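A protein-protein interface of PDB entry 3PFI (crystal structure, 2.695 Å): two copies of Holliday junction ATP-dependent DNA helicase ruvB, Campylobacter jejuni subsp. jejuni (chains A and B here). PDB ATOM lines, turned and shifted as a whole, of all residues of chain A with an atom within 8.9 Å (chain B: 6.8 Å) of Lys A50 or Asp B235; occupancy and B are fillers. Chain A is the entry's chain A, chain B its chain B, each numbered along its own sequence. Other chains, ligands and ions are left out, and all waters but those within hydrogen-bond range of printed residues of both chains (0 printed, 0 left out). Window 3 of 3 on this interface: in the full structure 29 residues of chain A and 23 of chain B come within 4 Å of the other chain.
NH2 of Arg A51 lies close to NH1 of Arg B231, 3.2 Å away. NH2 of Arg A51 lies within salt-bridge range of OD1 of Asp B232 (2.6 Å). The guanidinium group of Arg A51 is in salt-bridge range of the side-chain carboxylate of Asp B235 (2.5 Å).
The guanidinium group of Arg A51 is in salt-bridge range of the side-chain carboxylate of Glu A53 (3.6 Å). The side-chain amino group of Lys B202 lies within hydrogen-bond range of the backbone carbonyl oxygen of Arg B231. NH2 of Arg B231 is in salt-bridge range of OD1 of Asp B232 (3.6 Å). O of Phe B233 sits close to OD1 of Asn B237 (2.9 Å).
Among the printed residues, merely in contact across the chains: Phe A44 with Asp B232, Ala A47 with Asp B232, Val A43 with Val B236, Lys A50 with Asp B235 and Phe A44 with Phe B233.
Printed residues of chain B within 4 Å of Val A43: Val B236. Of the printed residues of chain B, Phe A44 touches Asp B232 and Phe B233. Lys A49 touches none of the printed residues of chain B. Lys A50 touches one residue of chain B. Of the printed residues of chain B, Arg A51 touches Arg B231, Asp B232 and Asp B235. Of the printed residues of chain A, Phe B233 touches Phe A44. No residue of chain A comes within 4 Å of Ala B234. Asp B235 touches just these residues of chain A: Lys A50 (3.7 Å) and Arg A51 (2.5 Å). The nearest printed residue of chain B that does not touch Phe A44 is Val B236 (5.6 Å).
Of the 13 printed residues of chain B, 5 touch a printed residue of chain A. Printed residues of chain A that touch a printed residue of chain B: Val A43, Phe A44, Ala A47, Lys A50 and Arg A51. Along chain A the printed residues that touch a printed residue of chain B span positions 43 to 51. Among the printed residues, 8 pairs touch across the chains.
No position is printed for both chains. Of the 8 pairs that touch across the chains among the printed residues, none has its exchanged pair printed and touching as well.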
ATOM      1  N   VAL A  43      27.875  11.920 -20.719  1.00  0.00           N
ATOM      2  CA  VAL A  43      26.562  11.282 -20.778  1.00  0.00           C
ATOM      3  C   VAL A  43      25.443  12.259 -20.439  1.00  0.00           C
ATOM      4  O   VAL A  43      24.444  12.322 -21.147  1.00  0.00           O
ATOM      5  CB  VAL A  43      26.460  10.073 -19.826  1.00  0.00           C
ATOM      6  CG1 VAL A  43      25.024   9.563 -19.763  1.00  0.00           C
ATOM      7  CG2 VAL A  43      27.404   8.970 -20.262  1.00  0.00           C
ATOM      8  N   PHE A  44      25.618  13.030 -19.370  1.00  0.00           N
ATOM      9  CA  PHE A  44      24.592  13.979 -18.944  1.00  0.00           C
ATOM     10  C   PHE A  44      24.462  15.145 -19.912  1.00  0.00           C
ATOM     11  O   PHE A  44      23.377  15.700 -20.080  1.00  0.00           O
ATOM     12  CB  PHE A  44      24.857  14.501 -17.525  1.00  0.00           C
ATOM     13  CG  PHE A  44      25.106  13.414 -16.520  1.00  0.00           C
ATOM     14  CD1 PHE A  44      24.253  12.329 -16.429  1.00  0.00           C
ATOM     15  CD2 PHE A  44      26.169  13.496 -15.639  1.00  0.00           C
ATOM     16  CE1 PHE A  44      24.480  11.327 -15.508  1.00  0.00           C
ATOM     17  CE2 PHE A  44      26.393  12.505 -14.708  1.00  0.00           C
ATOM     18  CZ  PHE A  44      25.547  11.418 -14.645  1.00  0.00           C
ATOM     19  N   ILE A  45      25.565  15.515 -20.552  1.00  0.00           N
ATOM     20  CA  ILE A  45      25.543  16.606 -21.514  1.00  0.00           C
ATOM     21  C   ILE A  45      24.756  16.197 -22.751  1.00  0.00           C
ATOM     22  O   ILE A  45      23.993  16.992 -23.300  1.00  0.00           O
ATOM     23  CB  ILE A  45      26.964  17.037 -21.910  1.00  0.00           C
ATOM     24  CG1 ILE A  45      27.641  17.744 -20.731  1.00  0.00           C
ATOM     25  CG2 ILE A  45      26.918  17.980 -23.098  1.00  0.00           C
ATOM     26  CD1 ILE A  45      29.115  18.020 -20.936  1.00  0.00           C
ATOM     27  N   ALA A  46      24.929  14.951 -23.182  1.00  0.00           N
ATOM     28  CA  ALA A  46      24.218  14.454 -24.355  1.00  0.00           C
ATOM     29  C   ALA A  46      22.725  14.421 -24.070  1.00  0.00           C
ATOM     30  O   ALA A  46      21.913  14.855 -24.888  1.00  0.00           O
ATOM     31  CB  ALA A  46      24.715  13.068 -24.732  1.00  0.00           C
ATOM     32  N   ALA A  47      22.379  13.913 -22.891  1.00  0.00           N
ATOM     33  CA  ALA A  47      20.988  13.796 -22.467  1.00  0.00           C
ATOM     34  C   ALA A  47      20.273  15.148 -22.450  1.00  0.00           C
ATOM     35  O   ALA A  47      19.227  15.313 -23.073  1.00  0.00           O
ATOM     36  CB  ALA A  47      20.923  13.147 -21.098  1.00  0.00           C
ATOM     37  N   ALA A  48      20.844  16.112 -21.738  1.00  0.00           N
ATOM     38  CA  ALA A  48      20.247  17.437 -21.633  1.00  0.00           C
ATOM     39  C   ALA A  48      19.971  18.027 -23.011  1.00  0.00           C
ATOM     40  O   ALA A  48      18.872  18.517 -23.278  1.00  0.00           O
ATOM     41  CB  ALA A  48      21.147  18.360 -20.835  1.00  0.00           C
ATOM     42  N   LYS A  49      20.969  17.976 -23.886  1.00  0.00           N
ATOM     43  CA  LYS A  49      20.819  18.520 -25.233  1.00  0.00           C
ATOM     44  C   LYS A  49      19.797  17.725 -26.033  1.00  0.00           C
ATOM     45  O   LYS A  49      18.951  18.305 -26.704  1.00  0.00           O
ATOM     46  CB  LYS A  49      22.171  18.596 -25.954  1.00  0.00           C
ATOM     47  CG  LYS A  49      23.140  19.569 -25.283  1.00  0.00           C
ATOM     48  CD  LYS A  49      24.395  19.852 -26.103  1.00  0.00           C
ATOM     49  CE  LYS A  49      25.270  18.630 -26.286  1.00  0.00           C
ATOM     50  NZ  LYS A  49      26.541  18.988 -26.982  1.00  0.00           N
ATOM     51  N   LYS A  50      19.862  16.401 -25.947  1.00  0.00           N
ATOM     52  CA  LYS A  50      18.902  15.550 -26.642  1.00  0.00           C
ATOM     53  C   LYS A  50      17.497  15.907 -26.164  1.00  0.00           C
ATOM     54  O   LYS A  50      16.550  15.979 -26.948  1.00  0.00           O
ATOM     55  CB  LYS A  50      19.198  14.076 -26.353  1.00  0.00           C
ATOM     56  CG  LYS A  50      18.267  13.084 -27.049  1.00  0.00           C
ATOM     57  CD  LYS A  50      18.668  11.644 -26.743  1.00  0.00           C
ATOM     58  CE  LYS A  50      17.775  10.638 -27.457  1.00  0.00           C
ATOM     59  NZ  LYS A  50      16.349  10.735 -27.037  1.00  0.00           N
ATOM     60  N   ARG A  51      17.396  16.150 -24.862  1.00  0.00           N
ATOM     61  CA  ARG A  51      16.145  16.495 -24.206  1.00  0.00           C
ATOM     62  C   ARG A  51      15.817  17.957 -24.497  1.00  0.00           C
ATOM     63  O   ARG A  51      14.737  18.441 -24.171  1.00  0.00           O
ATOM     64  CB  ARG A  51      16.328  16.316 -22.701  1.00  0.00           C
ATOM     65  CG  ARG A  51      15.085  15.957 -21.935  1.00  0.00           C
ATOM     66  CD  ARG A  51      15.291  16.120 -20.437  1.00  0.00           C
ATOM     67  NE  ARG A  51      16.650  15.808 -20.009  1.00  0.00           N
ATOM     68  CZ  ARG A  51      17.135  14.582 -19.841  1.00  0.00           C
ATOM     69  NH1 ARG A  51      16.380  13.521 -20.097  1.00  0.00           N
ATOM     70  NH2 ARG A  51      18.388  14.421 -19.439  1.00  0.00           N
ATOM     71  N   ASN A  52      16.776  18.654 -25.104  1.00  0.00           N
ATOM     72  CA  ASN A  52      16.655  20.070 -25.434  1.00  0.00           C
ATOM     73  C   ASN A  52      16.422  20.900 -24.168  1.00  0.00           C
ATOM     74  O   ASN A  52      15.541  21.756 -24.120  1.00  0.00           O
ATOM     75  CB  ASN A  52      15.550  20.302 -26.463  1.00  0.00           C
ATOM     76  CG  ASN A  52      15.601  21.695 -27.069  1.00  0.00           C
ATOM     77  OD1 ASN A  52      16.586  22.416 -26.913  1.00  0.00           O
ATOM     78  ND2 ASN A  52      14.543  22.074 -27.777  1.00  0.00           N
ATOM     79  N   GLU A  53      17.226  20.616 -23.144  1.00  0.00           N
ATOM     80  CA  GLU A  53      17.167  21.310 -21.858  1.00  0.00           C
ATOM     81  C   GLU A  53      18.582  21.581 -21.363  1.00  0.00           C
ATOM     82  O   GLU A  53      19.554  21.110 -21.954  1.00  0.00           O
ATOM     83  CB  GLU A  53      16.463  20.454 -20.804  1.00  0.00           C
ATOM     84  CG  GLU A  53      15.008  20.143 -21.064  1.00  0.00           C
ATOM     85  CD  GLU A  53      14.391  19.340 -19.928  1.00  0.00           C
ATOM     86  OE1 GLU A  53      15.138  18.961 -18.999  1.00  0.00           O
ATOM     87  OE2 GLU A  53      13.165  19.086 -19.959  1.00  0.00           O
ATOM     88  N   CYS A  54      18.688  22.334 -20.272  1.00  0.00           N
ATOM     89  CA  CYS A  54      19.981  22.627 -19.674  1.00  0.00           C
ATOM     90  C   CYS A  54      20.230  21.589 -18.585  1.00  0.00           C
ATOM     91  O   CYS A  54      19.291  20.967 -18.100  1.00  0.00           O
ATOM     92  CB  CYS A  54      20.012  24.037 -19.085  1.00  0.00           C
ATOM     93  SG  CYS A  54      18.954  24.280 -17.647  1.00  0.00           S
ATOM     94  N   LEU A  55      21.490  21.403 -18.206  1.00  0.00           N
ATOM     95  CA  LEU A  55      21.845  20.421 -17.183  1.00  0.00           C
ATOM     96  C   LEU A  55      21.278  20.765 -15.815  1.00  0.00           C
ATOM     97  O   LEU A  55      21.043  21.934 -15.505  1.00  0.00           O
ATOM     98  CB  LEU A  55      23.369  20.303 -17.037  1.00  0.00           C
ATOM     99  CG  LEU A  55      24.184  19.669 -18.162  1.00  0.00           C
ATOM    100  CD1 LEU A  55      23.968  20.405 -19.453  1.00  0.00           C
ATOM    101  CD2 LEU A  55      25.653  19.678 -17.806  1.00  0.00           C
ATOM    102  N   MET A  79      27.819  23.348 -23.518  1.00  0.00           N
ATOM    103  CA  MET A  79      26.386  23.635 -23.533  1.00  0.00           C
ATOM    104  C   MET A  79      26.038  24.902 -24.305  1.00  0.00           C
ATOM    105  O   MET A  79      24.892  25.337 -24.286  1.00  0.00           O
ATOM    106  CB  MET A  79      25.853  23.751 -22.103  1.00  0.00           C
ATOM    107  CG  MET A  79      25.851  22.437 -21.339  1.00  0.00           C
ATOM    108  SD  MET A  79      24.610  21.158 -22.129  1.00  0.00           S
ATOM    109  CE  MET A  79      22.943  22.123 -21.828  1.00  0.00           C
ATOM    110  N   LEU B 200       8.588  11.096 -15.794  1.00  0.00           N
ATOM    111  CA  LEU B 200       9.759  11.322 -16.635  1.00  0.00           C
ATOM    112  C   LEU B 200       9.677  10.458 -17.900  1.00  0.00           C
ATOM    113  O   LEU B 200      10.694  10.094 -18.489  1.00  0.00           O
ATOM    114  CB  LEU B 200      11.056  11.021 -15.875  1.00  0.00           C
ATOM    115  CG  LEU B 200      11.421  11.920 -14.691  1.00  0.00           C
ATOM    116  CD1 LEU B 200      12.783  11.512 -14.148  1.00  0.00           C
ATOM    117  CD2 LEU B 200      11.430  13.391 -15.095  1.00  0.00           C
ATOM    118  N   LYS B 202       9.222   7.324 -18.557  1.00  0.00           N
ATOM    119  CA  LYS B 202       9.994   6.081 -18.616  1.00  0.00           C
ATOM    120  C   LYS B 202       9.524   5.037 -17.609  1.00  0.00           C
ATOM    121  O   LYS B 202       9.107   5.372 -16.507  1.00  0.00           O
ATOM    122  CB  LYS B 202      11.493   6.353 -18.486  1.00  0.00           C
ATOM    123  CG  LYS B 202      12.048   7.065 -19.714  1.00  0.00           C
ATOM    124  CD  LYS B 202      13.552   7.103 -19.789  1.00  0.00           C
ATOM    125  CE  LYS B 202      13.971   7.661 -21.143  1.00  0.00           C
ATOM    126  NZ  LYS B 202      15.447   7.644 -21.332  1.00  0.00           N
ATOM    127  N   VAL B 230      20.067   8.125 -13.742  1.00  0.00           N
ATOM    128  CA  VAL B 230      19.839   6.878 -14.462  1.00  0.00           C
ATOM    129  C   VAL B 230      18.991   7.154 -15.710  1.00  0.00           C
ATOM    130  O   VAL B 230      19.186   6.516 -16.752  1.00  0.00           O
ATOM    131  CB  VAL B 230      19.157   5.818 -13.584  1.00  0.00           C
ATOM    132  CG1 VAL B 230      18.888   4.558 -14.394  1.00  0.00           C
ATOM    133  CG2 VAL B 230      20.022   5.500 -12.378  1.00  0.00           C
ATOM    134  N   ARG B 231      18.057   8.104 -15.611  1.00  0.00           N
ATOM    135  CA  ARG B 231      17.246   8.475 -16.766  1.00  0.00           C
ATOM    136  C   ARG B 231      18.169   8.861 -17.907  1.00  0.00           C
ATOM    137  O   ARG B 231      17.932   8.495 -19.060  1.00  0.00           O
ATOM    138  CB  ARG B 231      16.289   9.646 -16.484  1.00  0.00           C
ATOM    139  CG  ARG B 231      15.721  10.250 -17.800  1.00  0.00           C
ATOM    140  CD  ARG B 231      14.679  11.364 -17.631  1.00  0.00           C
ATOM    141  NE  ARG B 231      15.109  12.646 -17.050  1.00  0.00           N
ATOM    142  CZ  ARG B 231      16.359  13.058 -16.841  1.00  0.00           C
ATOM    143  NH1 ARG B 231      17.410  12.334 -17.190  1.00  0.00           N
ATOM    144  NH2 ARG B 231      16.561  14.247 -16.291  1.00  0.00           N
ATOM    145  N   ASP B 232      19.214   9.613 -17.579  1.00  0.00           N
ATOM    146  CA  ASP B 232      20.170  10.060 -18.581  1.00  0.00           C
ATOM    147  C   ASP B 232      20.879   8.895 -19.249  1.00  0.00           C
ATOM    148  O   ASP B 232      21.033   8.893 -20.468  1.00  0.00           O
ATOM    149  CB  ASP B 232      21.174  11.038 -17.977  1.00  0.00           C
ATOM    150  CG  ASP B 232      20.542  12.369 -17.633  1.00  0.00           C
ATOM    151  OD1 ASP B 232      19.338  12.532 -17.913  1.00  0.00           O
ATOM    152  OD2 ASP B 232      21.239  13.258 -17.104  1.00  0.00           O
ATOM    153  N   PHE B 233      21.310   7.904 -18.474  1.00  0.00           N
ATOM    154  CA  PHE B 233      21.959   6.742 -19.075  1.00  0.00           C
ATOM    155  C   PHE B 233      20.992   6.022 -20.005  1.00  0.00           C
ATOM    156  O   PHE B 233      21.401   5.448 -21.012  1.00  0.00           O
ATOM    157  CB  PHE B 233      22.545   5.801 -18.023  1.00  0.00           C
ATOM    158  CG  PHE B 233      23.903   6.219 -17.539  1.00  0.00           C
ATOM    159  CD1 PHE B 233      24.043   7.157 -16.534  1.00  0.00           C
ATOM    160  CD2 PHE B 233      25.043   5.675 -18.103  1.00  0.00           C
ATOM    161  CE1 PHE B 233      25.298   7.543 -16.094  1.00  0.00           C
ATOM    162  CE2 PHE B 233      26.299   6.058 -17.668  1.00  0.00           C
ATOM    163  CZ  PHE B 233      26.427   6.994 -16.663  1.00  0.00           C
ATOM    164  N   ALA B 234      19.709   6.066 -19.668  1.00  0.00           N
ATOM    165  CA  ALA B 234      18.681   5.469 -20.506  1.00  0.00           C
ATOM    166  C   ALA B 234      18.565   6.266 -21.817  1.00  0.00           C
ATOM    167  O   ALA B 234      18.574   5.682 -22.899  1.00  0.00           O
ATOM    168  CB  ALA B 234      17.348   5.440 -19.771  1.00  0.00           C
ATOM    169  N   ASP B 235      18.470   7.594 -21.711  1.00  0.00           N
ATOM    170  CA  ASP B 235      18.356   8.467 -22.891  1.00  0.00           C
ATOM    171  C   ASP B 235      19.448   8.222 -23.923  1.00  0.00           C
ATOM    172  O   ASP B 235      19.177   8.090 -25.120  1.00  0.00           O
ATOM    173  CB  ASP B 235      18.402   9.947 -22.495  1.00  0.00           C
ATOM    174  CG  ASP B 235      17.088  10.454 -21.946  1.00  0.00           C
ATOM    175  OD1 ASP B 235      16.093   9.709 -21.979  1.00  0.00           O
ATOM    176  OD2 ASP B 235      17.046  11.621 -21.507  1.00  0.00           O
ATOM    177  N   VAL B 236      20.683   8.182 -23.444  1.00  0.00           N
ATOM    178  CA  VAL B 236      21.839   7.972 -24.301  1.00  0.00           C
ATOM    179  C   VAL B 236      21.748   6.662 -25.069  1.00  0.00           C
ATOM    180  O   VAL B 236      22.337   6.534 -26.134  1.00  0.00           O
ATOM    181  CB  VAL B 236      23.144   8.003 -23.480  1.00  0.00           C
ATOM    182  CG1 VAL B 236      24.314   7.526 -24.315  1.00  0.00           C
ATOM    183  CG2 VAL B 236      23.388   9.409 -22.942  1.00  0.00           C
ATOM    184  N   ASN B 237      21.011   5.695 -24.536  1.00  0.00           N
ATOM    185  CA  ASN B 237      20.859   4.408 -25.204  1.00  0.00           C
ATOM    186  C   ASN B 237      19.463   4.222 -25.816  1.00  0.00           C
ATOM    187  O   ASN B 237      19.075   3.108 -26.166  1.00  0.00           O
ATOM    188  CB  ASN B 237      21.198   3.264 -24.242  1.00  0.00           C
ATOM    189  CG  ASN B 237      22.613   3.369 -23.680  1.00  0.00           C
ATOM    190  OD1 ASN B 237      23.043   4.436 -23.240  1.00  0.00           O
ATOM    191  ND2 ASN B 237      23.333   2.256 -23.675  1.00  0.00           N
ATOM    192  N   ASP B 238      18.726   5.324 -25.958  1.00  0.00           N
ATOM    193  CA  ASP B 238      17.381   5.304 -26.534  1.00  0.00           C
ATOM    194  C   ASP B 238      16.486   4.285 -25.842  1.00  0.00           C
ATOM    195  O   ASP B 238      15.686   3.613 -26.489  1.00  0.00           O
ATOM    196  CB  ASP B 238      17.436   4.986 -28.031  1.00  0.00           C
ATOM    197  CG  ASP B 238      18.295   5.965 -28.805  1.00  0.00           C
ATOM    198  OD1 ASP B 238      19.008   6.768 -28.170  1.00  0.00           O
ATOM    199  OD2 ASP B 238      18.264   5.923 -30.055  1.00  0.00           O
ATOM    200  N   GLU B 239      16.617   4.178 -24.526  1.00  0.00           N
ATOM    201  CA  GLU B 239      15.831   3.226 -23.760  1.00  0.00           C
ATOM    202  C   GLU B 239      14.734   3.899 -22.957  1.00  0.00           C
ATOM    203  O   GLU B 239      14.987   4.872 -22.249  1.00  0.00           O
ATOM    204  CB  GLU B 239      16.734   2.441 -22.811  1.00  0.00           C
ATOM    205  CG  GLU B 239      17.695   1.500 -23.509  1.00  0.00           C
ATOM    206  CD  GLU B 239      18.614   0.787 -22.539  1.00  0.00           C
ATOM    207  OE1 GLU B 239      18.812   1.302 -21.417  1.00  0.00           O
ATOM    208  OE2 GLU B 239      19.152  -0.282 -22.900  1.00  0.00           O
ATOM    209  N   GLU B 240      13.515   3.378 -23.084  1.00  0.00           N
ATOM    210  CA  GLU B 240      12.370   3.873 -22.327  1.00  0.00           C
ATOM    211  C   GLU B 240      12.207   3.046 -21.053  1.00  0.00           C
ATOM    212  O   GLU B 240      11.570   3.481 -20.098  1.00  0.00           O
ATOM    213  CB  GLU B 240      11.088   3.759 -23.142  1.00  0.00           C
ATOM    214  CG  GLU B 240      11.075   4.539 -24.435  1.00  0.00           C
ATOM    215  CD  GLU B 240       9.744   4.414 -25.161  1.00  0.00           C
ATOM    216  OE1 GLU B 240       9.604   4.980 -26.266  1.00  0.00           O
ATOM    217  OE2 GLU B 240       8.833   3.745 -24.629  1.00  0.00           O
